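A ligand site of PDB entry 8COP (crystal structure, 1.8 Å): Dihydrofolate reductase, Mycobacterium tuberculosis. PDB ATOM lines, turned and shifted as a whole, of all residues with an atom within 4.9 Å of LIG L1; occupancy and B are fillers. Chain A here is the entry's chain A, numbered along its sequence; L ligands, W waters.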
ATOM      1  N   ILE A   7      28.292 -10.881  11.030  1.00  0.00           N
ATOM      2  CA  ILE A   7      28.651 -11.129   9.654  1.00  0.00           C
ATOM      3  C   ILE A   7      28.995  -9.782   9.049  1.00  0.00           C
ATOM      4  O   ILE A   7      28.253  -8.818   9.229  1.00  0.00           O
ATOM      5  CB  ILE A   7      27.523 -11.853   8.905  1.00  0.00           C
ATOM      6  CG1 ILE A   7      27.938 -12.249   7.478  1.00  0.00           C
ATOM      7  CG2 ILE A   7      26.210 -11.093   9.005  1.00  0.00           C
ATOM      8  CD1 ILE A   7      26.846 -12.941   6.753  1.00  0.00           C
ATOM      9  N   TRP A   8      30.162  -9.699   8.411  1.00  0.00           N
ATOM     10  CA  TRP A   8      30.527  -8.479   7.706  1.00  0.00           C
ATOM     11  C   TRP A   8      31.402  -8.841   6.534  1.00  0.00           C
ATOM     12  O   TRP A   8      31.947  -9.943   6.448  1.00  0.00           O
ATOM     13  CB  TRP A   8      31.288  -7.460   8.580  1.00  0.00           C
ATOM     14  CG  TRP A   8      32.665  -7.857   9.103  1.00  0.00           C
ATOM     15  CD1 TRP A   8      33.833  -7.771   8.426  1.00  0.00           C
ATOM     16  CD2 TRP A   8      32.993  -8.358  10.406  1.00  0.00           C
ATOM     17  NE1 TRP A   8      34.879  -8.196   9.210  1.00  0.00           N
ATOM     18  CE2 TRP A   8      34.388  -8.564  10.433  1.00  0.00           C
ATOM     19  CE3 TRP A   8      32.249  -8.667  11.547  1.00  0.00           C
ATOM     20  CZ2 TRP A   8      35.044  -9.052  11.534  1.00  0.00           C
ATOM     21  CZ3 TRP A   8      32.907  -9.144  12.638  1.00  0.00           C
ATOM     22  CH2 TRP A   8      34.293  -9.345  12.626  1.00  0.00           C
ATOM     23  N   ALA A   9      31.542  -7.883   5.632  1.00  0.00           N
ATOM     24  CA  ALA A   9      32.520  -7.925   4.558  1.00  0.00           C
ATOM     25  C   ALA A   9      33.481  -6.782   4.785  1.00  0.00           C
ATOM     26  O   ALA A   9      33.057  -5.667   5.075  1.00  0.00           O
ATOM     27  CB  ALA A   9      31.862  -7.769   3.190  1.00  0.00           C
ATOM     28  N   ILE A  16      34.897  -1.458   6.394  1.00  0.00           N
ATOM     29  CA  ILE A  16      33.603  -2.001   5.997  1.00  0.00           C
ATOM     30  C   ILE A  16      32.710  -0.961   5.327  1.00  0.00           C
ATOM     31  O   ILE A  16      31.772  -1.342   4.601  1.00  0.00           O
ATOM     32  CB  ILE A  16      32.865  -2.631   7.203  1.00  0.00           C
ATOM     33  CG1 ILE A  16      32.692  -1.598   8.316  1.00  0.00           C
ATOM     34  CG2 ILE A  16      33.616  -3.861   7.744  1.00  0.00           C
ATOM     35  CD1 ILE A  16      31.452  -1.800   9.183  1.00  0.00           C
ATOM     36  N   GLY A  17      32.944   0.324   5.557  1.00  0.00           N
ATOM     37  CA  GLY A  17      32.034   1.333   5.055  1.00  0.00           C
ATOM     38  C   GLY A  17      32.708   2.679   5.009  1.00  0.00           C
ATOM     39  O   GLY A  17      33.696   2.932   5.706  1.00  0.00           O
ATOM     40  N   ARG A  18      32.136   3.566   4.194  1.00  0.00           N
ATOM     41  CA  ARG A  18      32.686   4.894   4.004  1.00  0.00           C
ATOM     42  C   ARG A  18      31.560   5.760   3.454  1.00  0.00           C
ATOM     43  O   ARG A  18      30.727   5.284   2.683  1.00  0.00           O
ATOM     44  CB  ARG A  18      33.872   4.829   3.034  1.00  0.00           C
ATOM     45  CG  ARG A  18      34.609   6.119   2.805  1.00  0.00           C
ATOM     46  CD  ARG A  18      35.830   5.847   1.930  1.00  0.00           C
ATOM     47  NE  ARG A  18      36.931   5.272   2.693  1.00  0.00           N
ATOM     48  CZ  ARG A  18      38.101   4.898   2.160  1.00  0.00           C
ATOM     49  NH1 ARG A  18      38.332   5.102   0.857  1.00  0.00           N
ATOM     50  NH2 ARG A  18      39.047   4.359   2.922  1.00  0.00           N
ATOM     51  N   GLY A  20      28.944   6.572   4.801  1.00  0.00           N
ATOM     52  CA  GLY A  20      27.670   5.954   5.121  1.00  0.00           C
ATOM     53  C   GLY A  20      27.202   4.973   4.067  1.00  0.00           C
ATOM     54  O   GLY A  20      26.002   4.935   3.764  1.00  0.00           O
ATOM     55  N   ASP A  21      28.106   4.165   3.522  1.00  0.00           N
ATOM     56  CA  ASP A  21      27.778   3.233   2.445  1.00  0.00           C
ATOM     57  C   ASP A  21      29.022   2.352   2.223  1.00  0.00           C
ATOM     58  O   ASP A  21      29.959   2.371   3.031  1.00  0.00           O
ATOM     59  CB  ASP A  21      27.296   4.028   1.233  1.00  0.00           C
ATOM     60  CG  ASP A  21      26.619   3.190   0.205  1.00  0.00           C
ATOM     61  OD1 ASP A  21      26.652   1.947   0.286  1.00  0.00           O
ATOM     62  OD2 ASP A  21      25.932   3.814  -0.634  1.00  0.00           O
ATOM     63  N   ILE A  22      29.030   1.546   1.155  1.00  0.00           N
ATOM     64  CA  ILE A  22      30.075   0.518   1.017  1.00  0.00           C
ATOM     65  C   ILE A  22      30.735   0.615  -0.344  1.00  0.00           C
ATOM     66  O   ILE A  22      30.031   0.647  -1.362  1.00  0.00           O
ATOM     67  CB  ILE A  22      29.502  -0.887   1.200  1.00  0.00           C
ATOM     68  CG1 ILE A  22      28.863  -1.039   2.567  1.00  0.00           C
ATOM     69  CG2 ILE A  22      30.608  -1.910   1.124  1.00  0.00           C
ATOM     70  CD1 ILE A  22      27.834  -2.151   2.593  1.00  0.00           C
ATOM     71  N   TRP A  24      32.066  -1.317  -2.495  1.00  0.00           N
ATOM     72  CA  TRP A  24      32.135  -2.522  -3.303  1.00  0.00           C
ATOM     73  C   TRP A  24      30.752  -3.151  -3.358  1.00  0.00           C
ATOM     74  O   TRP A  24      29.867  -2.816  -2.560  1.00  0.00           O
ATOM     75  CB  TRP A  24      33.180  -3.514  -2.786  1.00  0.00           C
ATOM     76  CG  TRP A  24      32.901  -4.001  -1.417  1.00  0.00           C
ATOM     77  CD1 TRP A  24      31.954  -4.903  -1.032  1.00  0.00           C
ATOM     78  CD2 TRP A  24      33.626  -3.653  -0.227  1.00  0.00           C
ATOM     79  NE1 TRP A  24      32.007  -5.098   0.329  1.00  0.00           N
ATOM     80  CE2 TRP A  24      33.041  -4.349   0.846  1.00  0.00           C
ATOM     81  CE3 TRP A  24      34.710  -2.798   0.029  1.00  0.00           C
ATOM     82  CZ2 TRP A  24      33.494  -4.220   2.152  1.00  0.00           C
ATOM     83  CZ3 TRP A  24      35.154  -2.668   1.335  1.00  0.00           C
ATOM     84  CH2 TRP A  24      34.547  -3.377   2.367  1.00  0.00           C
ATOM     85  N   GLY A  45      22.563  -1.224  13.076  1.00  0.00           N
ATOM     86  CA  GLY A  45      22.522   0.135  13.577  1.00  0.00           C
ATOM     87  C   GLY A  45      21.571   1.002  12.791  1.00  0.00           C
ATOM     88  O   GLY A  45      21.312   0.769  11.611  1.00  0.00           O
ATOM     89  N   ARG A  46      21.013   2.005  13.460  1.00  0.00           N
ATOM     90  CA  ARG A  46      20.132   2.933  12.771  1.00  0.00           C
ATOM     91  C   ARG A  46      20.814   3.532  11.562  1.00  0.00           C
ATOM     92  O   ARG A  46      20.192   3.745  10.520  1.00  0.00           O
ATOM     93  CB  ARG A  46      19.712   4.053  13.705  1.00  0.00           C
ATOM     94  CG  ARG A  46      18.580   4.821  13.127  1.00  0.00           C
ATOM     95  CD  ARG A  46      18.825   6.282  13.171  1.00  0.00           C
ATOM     96  NE  ARG A  46      19.816   6.620  12.159  1.00  0.00           N
ATOM     97  CZ  ARG A  46      20.690   7.603  12.270  1.00  0.00           C
ATOM     98  NH1 ARG A  46      20.719   8.329  13.373  1.00  0.00           N
ATOM     99  NH2 ARG A  46      21.532   7.841  11.286  1.00  0.00           N
ATOM    100  N   ARG A  47      22.116   3.803  11.676  1.00  0.00           N
ATOM    101  CA  ARG A  47      22.795   4.454  10.581  1.00  0.00           C
ATOM    102  C   ARG A  47      23.012   3.500   9.415  1.00  0.00           C
ATOM    103  O   ARG A  47      23.354   3.953   8.316  1.00  0.00           O
ATOM    104  CB  ARG A  47      24.097   5.054  11.133  1.00  0.00           C
ATOM    105  CG  ARG A  47      24.850   5.974  10.202  1.00  0.00           C
ATOM    106  CD  ARG A  47      26.135   6.483  10.897  1.00  0.00           C
ATOM    107  NE  ARG A  47      25.911   7.337  12.065  1.00  0.00           N
ATOM    108  CZ  ARG A  47      26.899   7.778  12.837  1.00  0.00           C
ATOM    109  NH1 ARG A  47      28.150   7.473  12.522  1.00  0.00           N
ATOM    110  NH2 ARG A  47      26.651   8.542  13.906  1.00  0.00           N
ATOM    111  N   THR A  48      22.790   2.196   9.625  1.00  0.00           N
ATOM    112  CA  THR A  48      22.692   1.183   8.568  1.00  0.00           C
ATOM    113  C   THR A  48      21.275   1.041   8.000  1.00  0.00           C
ATOM    114  O   THR A  48      21.105   0.857   6.796  1.00  0.00           O
ATOM    115  CB  THR A  48      23.178  -0.175   9.112  1.00  0.00           C
ATOM    116  OG1 THR A  48      24.593  -0.125   9.321  1.00  0.00           O
ATOM    117  CG2 THR A  48      22.843  -1.320   8.148  1.00  0.00           C
ATOM    118  N   LEU A  67      18.749  -0.689  15.856  1.00  0.00           N
ATOM    119  CA  LEU A  67      19.135  -0.235  17.177  1.00  0.00           C
ATOM    120  C   LEU A  67      19.380   1.276  17.105  1.00  0.00           C
ATOM    121  O   LEU A  67      20.157   1.737  16.258  1.00  0.00           O
ATOM    122  CB  LEU A  67      20.348  -1.010  17.676  1.00  0.00           C
ATOM    123  CG  LEU A  67      21.142  -0.437  18.836  1.00  0.00           C
ATOM    124  CD1 LEU A  67      20.366  -0.690  20.101  1.00  0.00           C
ATOM    125  CD2 LEU A  67      22.488  -1.109  18.935  1.00  0.00           C
ATOM    126  N   SER A  68      18.677   2.034  17.952  1.00  0.00           N
ATOM    127  CA  SER A  68      18.721   3.501  17.971  1.00  0.00           C
ATOM    128  C   SER A  68      18.550   4.020  19.384  1.00  0.00           C
ATOM    129  O   SER A  68      17.981   3.349  20.259  1.00  0.00           O
ATOM    130  CB  SER A  68      17.629   4.124  17.092  1.00  0.00           C
ATOM    131  OG  SER A  68      17.613   5.543  17.186  1.00  0.00           O
ATOM    132  N   ARG A  69      19.063   5.217  19.604  1.00  0.00           N
ATOM    133  CA  ARG A  69      18.821   5.967  20.833  1.00  0.00           C
ATOM    134  C   ARG A  69      17.454   6.637  20.793  1.00  0.00           C
ATOM    135  O   ARG A  69      16.767   6.717  21.806  1.00  0.00           O
ATOM    136  CB  ARG A  69      19.902   7.034  20.996  1.00  0.00           C
ATOM    137  CG  ARG A  69      21.274   6.460  21.103  1.00  0.00           C
ATOM    138  CD  ARG A  69      21.832   6.485  22.463  1.00  0.00           C
ATOM    139  NE  ARG A  69      22.944   5.563  22.506  1.00  0.00           N
ATOM    140  CZ  ARG A  69      24.188   5.889  22.202  1.00  0.00           C
ATOM    141  NH1 ARG A  69      24.470   7.111  21.756  1.00  0.00           N
ATOM    142  NH2 ARG A  69      25.140   4.981  22.272  1.00  0.00           N
ATOM    143  N   GLN A  70      17.085   7.145  19.611  1.00  0.00           N
ATOM    144  CA  GLN A  70      15.810   7.805  19.382  1.00  0.00           C
ATOM    145  C   GLN A  70      14.670   6.972  19.939  1.00  0.00           C
ATOM    146  O   GLN A  70      14.335   5.914  19.394  1.00  0.00           O
ATOM    147  CB  GLN A  70      15.608   8.018  17.879  1.00  0.00           C
ATOM    148  CG  GLN A  70      16.212   9.284  17.354  1.00  0.00           C
ATOM    149  CD  GLN A  70      15.982   9.448  15.877  1.00  0.00           C
ATOM    150  OE1 GLN A  70      14.865   9.713  15.439  1.00  0.00           O
ATOM    151  NE2 GLN A  70      17.047   9.277  15.076  1.00  0.00           N
ATOM    152  N   VAL A  81      14.824  -0.738  18.888  1.00  0.00           N
ATOM    153  CA  VAL A  81      15.082  -0.982  20.299  1.00  0.00           C
ATOM    154  C   VAL A  81      16.299  -0.171  20.686  1.00  0.00           C
ATOM    155  O   VAL A  81      17.236  -0.016  19.888  1.00  0.00           O
ATOM    156  CB  VAL A  81      15.303  -2.481  20.615  1.00  0.00           C
ATOM    157  CG1 VAL A  81      14.075  -3.291  20.238  1.00  0.00           C
ATOM    158  CG2 VAL A  81      16.548  -3.018  19.940  1.00  0.00           C
ATOM    159  N   GLY A  82      16.286   0.369  21.903  1.00  0.00           N
ATOM    160  CA  GLY A  82      17.335   1.218  22.419  1.00  0.00           C
ATOM    161  C   GLY A  82      18.485   0.493  23.051  1.00  0.00           C
ATOM    162  O   GLY A  82      19.479   1.121  23.407  1.00  0.00           O
ATOM    163  N   SER A  83      18.393  -0.826  23.193  1.00  0.00           N
ATOM    164  CA  SER A  83      19.473  -1.604  23.758  1.00  0.00           C
ATOM    165  C   SER A  83      19.571  -2.934  23.051  1.00  0.00           C
ATOM    166  O   SER A  83      18.586  -3.458  22.533  1.00  0.00           O
ATOM    167  CB  SER A  83      19.268  -1.819  25.251  1.00  0.00           C
ATOM    168  OG  SER A  83      19.319  -0.571  25.916  1.00  0.00           O
ATOM    169  N   ILE A  96      24.329  -7.330  11.652  1.00  0.00           N
ATOM    170  CA  ILE A  96      24.698  -7.160  10.240  1.00  0.00           C
ATOM    171  C   ILE A  96      25.278  -5.777   9.954  1.00  0.00           C
ATOM    172  O   ILE A  96      25.498  -5.451   8.792  1.00  0.00           O
ATOM    173  CB  ILE A  96      23.511  -7.463   9.323  1.00  0.00           C
ATOM    174  CG1 ILE A  96      22.365  -6.479   9.575  1.00  0.00           C
ATOM    175  CG2 ILE A  96      23.036  -8.883   9.608  1.00  0.00           C
ATOM    176  CD1 ILE A  96      21.285  -6.577   8.548  1.00  0.00           C
ATOM    177  N   GLY A  97      25.545  -4.972  10.969  1.00  0.00           N
ATOM    178  CA  GLY A  97      26.280  -3.747  10.785  1.00  0.00           C
ATOM    179  C   GLY A  97      25.668  -2.579  11.537  1.00  0.00           C
ATOM    180  O   GLY A  97      24.564  -2.654  12.086  1.00  0.00           O
ATOM    181  N   GLY A  98      26.429  -1.488  11.574  1.00  0.00           N
ATOM    182  CA  GLY A  98      27.772  -1.434  11.039  1.00  0.00           C
ATOM    183  C   GLY A  98      28.832  -1.276  12.121  1.00  0.00           C
ATOM    184  O   GLY A  98      28.786  -1.965  13.138  1.00  0.00           O
ATOM    185  N   GLY A  99      29.771  -0.347  11.918  1.00  0.00           N
ATOM    186  CA  GLY A  99      30.939  -0.281  12.785  1.00  0.00           C
ATOM    187  C   GLY A  99      30.598  -0.104  14.256  1.00  0.00           C
ATOM    188  O   GLY A  99      31.187  -0.765  15.121  1.00  0.00           O
ATOM    189  N   GLN A 100      29.658   0.779  14.566  1.00  0.00           N
ATOM    190  CA  GLN A 100      29.328   0.959  15.977  1.00  0.00           C
ATOM    191  C   GLN A 100      28.714  -0.301  16.563  1.00  0.00           C
ATOM    192  O   GLN A 100      29.157  -0.798  17.587  1.00  0.00           O
ATOM    193  CB  GLN A 100      28.403   2.165  16.183  1.00  0.00           C
ATOM    194  CG  GLN A 100      28.973   3.468  15.640  1.00  0.00           C
ATOM    195  CD  GLN A 100      28.172   4.699  16.031  1.00  0.00           C
ATOM    196  OE1 GLN A 100      27.115   4.608  16.670  1.00  0.00           O
ATOM    197  NE2 GLN A 100      28.696   5.862  15.676  1.00  0.00           N
ATOM    198  N   VAL A 101      27.697  -0.847  15.892  1.00  0.00           N
ATOM    199  CA  VAL A 101      27.017  -2.019  16.413  1.00  0.00           C
ATOM    200  C   VAL A 101      27.915  -3.251  16.455  1.00  0.00           C
ATOM    201  O   VAL A 101      27.731  -4.108  17.325  1.00  0.00           O
ATOM    202  CB  VAL A 101      25.743  -2.233  15.581  1.00  0.00           C
ATOM    203  CG1 VAL A 101      24.994  -3.460  16.046  1.00  0.00           C
ATOM    204  CG2 VAL A 101      24.883  -1.004  15.740  1.00  0.00           C
ATOM    205  N   TYR A 102      28.932  -3.348  15.589  1.00  0.00           N
ATOM    206  CA  TYR A 102      29.836  -4.480  15.640  1.00  0.00           C
ATOM    207  C   TYR A 102      30.564  -4.532  16.978  1.00  0.00           C
ATOM    208  O   TYR A 102      30.470  -5.524  17.699  1.00  0.00           O
ATOM    209  CB  TYR A 102      30.859  -4.443  14.504  1.00  0.00           C
ATOM    210  CG  TYR A 102      30.308  -4.909  13.178  1.00  0.00           C
ATOM    211  CD1 TYR A 102      30.708  -4.295  11.993  1.00  0.00           C
ATOM    212  CD2 TYR A 102      29.359  -5.915  13.114  1.00  0.00           C
ATOM    213  CE1 TYR A 102      30.179  -4.684  10.785  1.00  0.00           C
ATOM    214  CE2 TYR A 102      28.838  -6.316  11.914  1.00  0.00           C
ATOM    215  CZ  TYR A 102      29.259  -5.697  10.750  1.00  0.00           C
ATOM    216  OH  TYR A 102      28.746  -6.048   9.535  1.00  0.00           O
ATOM    217  N   LEU A 104      29.928  -3.195  19.620  1.00  0.00           N
ATOM    218  CA  LEU A 104      28.984  -3.254  20.736  1.00  0.00           C
ATOM    219  C   LEU A 104      28.547  -4.683  21.042  1.00  0.00           C
ATOM    220  O   LEU A 104      28.295  -5.024  22.202  1.00  0.00           O
ATOM    221  CB  LEU A 104      27.762  -2.400  20.394  1.00  0.00           C
ATOM    222  CG  LEU A 104      26.712  -2.122  21.465  1.00  0.00           C
ATOM    223  CD1 LEU A 104      27.340  -1.508  22.694  1.00  0.00           C
ATOM    224  CD2 LEU A 104      25.648  -1.253  20.877  1.00  0.00           C
ATOM    225  N   ALA A 128      34.179   3.407   8.747  1.00  0.00           N
ATOM    226  CA  ALA A 128      33.799   2.353   9.686  1.00  0.00           C
ATOM    227  C   ALA A 128      34.634   1.095   9.434  1.00  0.00           C
ATOM    228  O   ALA A 128      34.923   0.747   8.289  1.00  0.00           O
ATOM    229  CB  ALA A 128      32.308   2.042   9.575  1.00  0.00           C
HETATM  230  P1  LIG L   1      25.911   1.951  12.592  1.00  0.00           P
HETATM  231  O1  LIG L   1      26.740   1.277  13.622  1.00  0.00           O
HETATM  232  O2  LIG L   1      25.475   1.265  11.342  1.00  0.00           O
HETATM  233  O3  LIG L   1      24.564   2.546  13.270  1.00  0.00           O
HETATM  234  C1  LIG L   1      25.000   3.449  14.237  1.00  0.00           C
HETATM  235  C2  LIG L   1      23.790   3.784  15.067  1.00  0.00           C
HETATM  236  O4  LIG L   1      23.625   2.811  16.068  1.00  0.00           O
HETATM  237  C3  LIG L   1      23.975   5.115  15.802  1.00  0.00           C
HETATM  238  O5  LIG L   1      23.705   6.162  14.916  1.00  0.00           O
HETATM  239  C4  LIG L   1      22.841   5.013  16.849  1.00  0.00           C
HETATM  240  O6  LIG L   1      21.650   5.255  16.338  1.00  0.00           O
HETATM  241  C5  LIG L   1      22.858   3.441  17.114  1.00  0.00           C
HETATM  242  N1  LIG L   1      23.426   3.043  18.400  1.00  0.00           N
HETATM  243  C6  LIG L   1      24.761   2.862  18.739  1.00  0.00           C
HETATM  244  N2  LIG L   1      24.935   2.470  20.017  1.00  0.00           N
HETATM  245  C7  LIG L   1      23.639   2.399  20.531  1.00  0.00           C
HETATM  246  C8  LIG L   1      23.153   2.058  21.786  1.00  0.00           C
HETATM  247  N3  LIG L   1      24.027   1.714  22.793  1.00  0.00           N
HETATM  248  N4  LIG L   1      21.840   2.051  22.065  1.00  0.00           N
HETATM  249  C9  LIG L   1      21.019   2.408  21.030  1.00  0.00           C
HETATM  250  N5  LIG L   1      21.333   2.748  19.770  1.00  0.00           N
HETATM  251  C10 LIG L   1      22.694   2.743  19.542  1.00  0.00           C
HETATM  252  O7  LIG L   1      26.787   3.271  12.209  1.00  0.00           O
HETATM  253  P2  LIG L   1      28.167   2.991  11.477  1.00  0.00           P
HETATM  254  O8  LIG L   1      29.159   2.498  12.445  1.00  0.00           O
HETATM  255  O9  LIG L   1      28.521   4.129  10.554  1.00  0.00           O
HETATM  256  O10 LIG L   1      28.040   1.683  10.354  1.00  0.00           O
HETATM  257  C11 LIG L   1      27.513   2.207   9.180  1.00  0.00           C
HETATM  258  C12 LIG L   1      28.493   1.935   8.048  1.00  0.00           C
HETATM  259  O11 LIG L   1      28.785   0.530   7.971  1.00  0.00           O
HETATM  260  C13 LIG L   1      27.850   2.362   6.692  1.00  0.00           C
HETATM  261  O12 LIG L   1      28.878   2.884   5.946  1.00  0.00           O
HETATM  262  C14 LIG L   1      27.434   1.058   6.094  1.00  0.00           C
HETATM  263  O13 LIG L   1      27.507   1.103   4.705  1.00  0.00           O
HETATM  264  C15 LIG L   1      28.603   0.144   6.641  1.00  0.00           C
HETATM  265  N6  LIG L   1      28.207  -1.303   6.614  1.00  0.00           N
HETATM  266  C16 LIG L   1      29.076  -2.261   6.117  1.00  0.00           C
HETATM  267  C17 LIG L   1      28.780  -3.587   6.253  1.00  0.00           C
HETATM  268  C18 LIG L   1      29.731  -4.542   5.687  1.00  0.00           C
HETATM  269  O14 LIG L   1      30.683  -4.232   4.953  1.00  0.00           O
HETATM  270  N7  LIG L   1      29.554  -5.873   6.007  1.00  0.00           N
HETATM  271  C19 LIG L   1      27.559  -4.051   6.938  1.00  0.00           C
HETATM  272  C20 LIG L   1      26.633  -2.966   7.244  1.00  0.00           C
HETATM  273  C21 LIG L   1      26.961  -1.685   7.095  1.00  0.00           C
HETATM  274  P3  LIG L   1      20.886   6.877  16.601  1.00  0.00           P
HETATM  275  O15 LIG L   1      21.818   7.659  15.734  1.00  0.00           O
HETATM  276  O16 LIG L   1      19.437   6.733  16.123  1.00  0.00           O
HETATM  277  O17 LIG L   1      21.102   6.929  18.076  1.00  0.00           O
HETATM  278  C1  LG2 L   2      25.581  -4.967   1.136  1.00  0.00           C
HETATM  279  C2  LG2 L   2      25.227  -5.699   0.034  1.00  0.00           C
HETATM  280  C3  LG2 L   2      22.134  -4.371   4.743  1.00  0.00           C
HETATM  281  C4  LG2 L   2      28.288  -9.272   4.567  1.00  0.00           C
HETATM  282  C5  LG2 L   2      26.719  -7.692   3.552  1.00  0.00           C
HETATM  283  C6  LG2 L   2      26.276  -7.350   4.824  1.00  0.00           C
HETATM  284  C7  LG2 L   2      26.881  -8.027   5.857  1.00  0.00           C
HETATM  285  C8  LG2 L   2      25.189  -6.319   5.131  1.00  0.00           C
HETATM  286  C9  LG2 L   2      24.334  -5.537   5.394  1.00  0.00           C
HETATM  287  C10 LG2 L   2      26.166  -7.024   2.278  1.00  0.00           C
HETATM  288  C11 LG2 L   2      23.266  -4.505   5.763  1.00  0.00           C
HETATM  289  C12 LG2 L   2      26.057  -5.620   2.259  1.00  0.00           C
HETATM  290  C13 LG2 L   2      25.329  -7.078   0.015  1.00  0.00           C
HETATM  291  C14 LG2 L   2      25.802  -7.751   1.137  1.00  0.00           C
HETATM  292  C15 LG2 L   2      22.665  -4.427  -3.067  1.00  0.00           C
HETATM  293  C16 LG2 L   2      23.216  -3.298   4.836  1.00  0.00           C
HETATM  294  N1  LG2 L   2      27.835  -8.934   5.787  1.00  0.00           N
HETATM  295  N2  LG2 L   2      27.709  -8.620   3.541  1.00  0.00           N
HETATM  296  N3  LG2 L   2      26.409  -7.675   7.189  1.00  0.00           N
HETATM  297  N4  LG2 L   2      29.338 -10.277   4.381  1.00  0.00           N
HETATM  298  N5  LG2 L   2      24.743  -4.970  -1.123  1.00  0.00           N
HETATM  299  O1  LG2 L   2      22.721  -6.579  -1.433  1.00  0.00           O
HETATM  300  O2  LG2 L   2      24.326  -6.614  -3.103  1.00  0.00           O
HETATM  301  S1  LG2 L   2      23.638  -5.701  -2.193  1.00  0.00           S
HETATM  302  O   HOH W   1      30.215   5.303   9.085  1.00  0.00           O
HETATM  303  O   HOH W   2      24.843  -0.797   3.924  1.00  0.00           O
HETATM  304  O   HOH W   3      30.759   5.242   6.584  1.00  0.00           O
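O of Ala 9 lies close to O14 of LIG L1 (2.8 Å). The backbone carbonyl oxygen (O) of Ile 16 lies close to an oxygen (O14) of LIG L1, at 3.1 Å. O of Gly 82 lies close to N4 of LIG L1, 2.9 Å away. Residues that only touch LIG L1: Ile 96 (3.1 Å), Gly 45 (3.2 Å), Trp 8 (3.3 Å), Gly 20 (3.3 Å), Leu 67 (3.3 Å), Ile 22 (3.3 Å), Tyr 102 (3.5 Å), Gly 17 (3.6 Å), Gly 97 (3.6 Å), Gln 70 (3.6 Å), Arg 18 (3.8 Å), Leu 104 (3.9 Å) and Trp 24 (3.97 Å). Hydrophobic or aromatic side chains within 4 Å of LIG L1: Trp 8, Ile 16, Ile 22, Trp 24, Leu 67, Val 101 and Leu 104. Of the 30 residues printed, 26 come within 4 Å of LIG L1. Along chain A the residues within 4 Å of LIG L1 span positions 8 to 104. The nearest printed residue that does not touch LIG L1 is Ala 128 (4.1 Å).
Water W3 lies within hydrogen-bond range of the backbone NH of Gly 20, an oxygen (O12) of LIG L1 and the backbone NH of Arg 18.
N of Ala 128 is in hydrogen-bond range of O of Gly 17. The backbone NH (N) of Ile 16 lies within hydrogen-bond range of the backbone carbonyl oxygen (O) of Ala 128 (2.9 Å). OH of Tyr 102 sits at hydrogen-bond distance from O of Ile 7. The backbone carbonyl oxygen of Ile 96 lies within hydrogen-bond range of the side-chain hydroxyl of Tyr 102 (3.4 Å). OG1 of Thr 48 is in hydrogen-bond range of N of Gly 98 (3.2 Å). The backbone carbonyl oxygen (O) of Gly 97 is in hydrogen-bond range of the backbone NH (N) of Gly 45, 2.7 Å away. O of Val 81 is in hydrogen-bond range of N of Ser 68 (3.2 Å). The backbone carbonyl oxygen of Leu 67 lies within hydrogen-bond range of the backbone NH of Arg 46 (2.9 Å).
The backbone NH (N) of Thr 48 lies within hydrogen-bond range of an oxygen (O2) of LIG L1 (3.3 Å). N of Val 101 lies within hydrogen-bond range of O1 of LIG L1 (3.3 Å). The side-chain hydroxyl (OG1) of Thr 48 sits at hydrogen-bond distance from an oxygen (O2) of LIG L1, 2.6 Å away. The backbone NH (N) of Gly 99 sits at hydrogen-bond distance from an oxygen (O8) of LIG L1 (3.0 Å). The backbone NH (N) of Ser 68 lies close to a nitrogen (N5) of LIG L1. O16 of LIG L1 lies within hydrogen-bond range of OG of Ser 68. The backbone NH (N) of Gly 98 sits at hydrogen-bond distance from an oxygen (O2) of LIG L1. The backbone carbonyl oxygen of Asp 21 is in hydrogen-bond range of an oxygen (O12) of LIG L1 (3.2 Å). NH1 of Arg 46 lies within salt-bridge range of O15 of LIG L1 (2.7 Å). N of Arg 47 lies within hydrogen-bond range of O3 of LIG L1, 3.2 Å away. The backbone carbonyl oxygen (O) of Ile 7 sits at hydrogen-bond distance from a nitrogen (N3) of LG2 L2 (3.0 Å). The backbone NH (N) of Arg 69 sits close to an oxygen (O17) of LIG L1 (3.1 Å). An oxygen (O9) of LIG L1 lies within salt-bridge range of the guanidinium group (NH1) of Arg 47 (3.9 Å). The backbone NH (N) of Asp 21 is in hydrogen-bond range of an oxygen (O12) of LIG L1, 2.8 Å away. The backbone carbonyl oxygen (O) of Ile 96 is in hydrogen-bond range of a nitrogen (N3) of LG2 L2, at 2.9 Å. NH2 of Arg 69 is in hydrogen-bond range of N2 of LIG L1 (3.4 Å). N of Gln 100 sits at hydrogen-bond distance from O8 of LIG L1, 2.8 Å away. O of Trp 8 lies close to N4 of LG2 L2.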
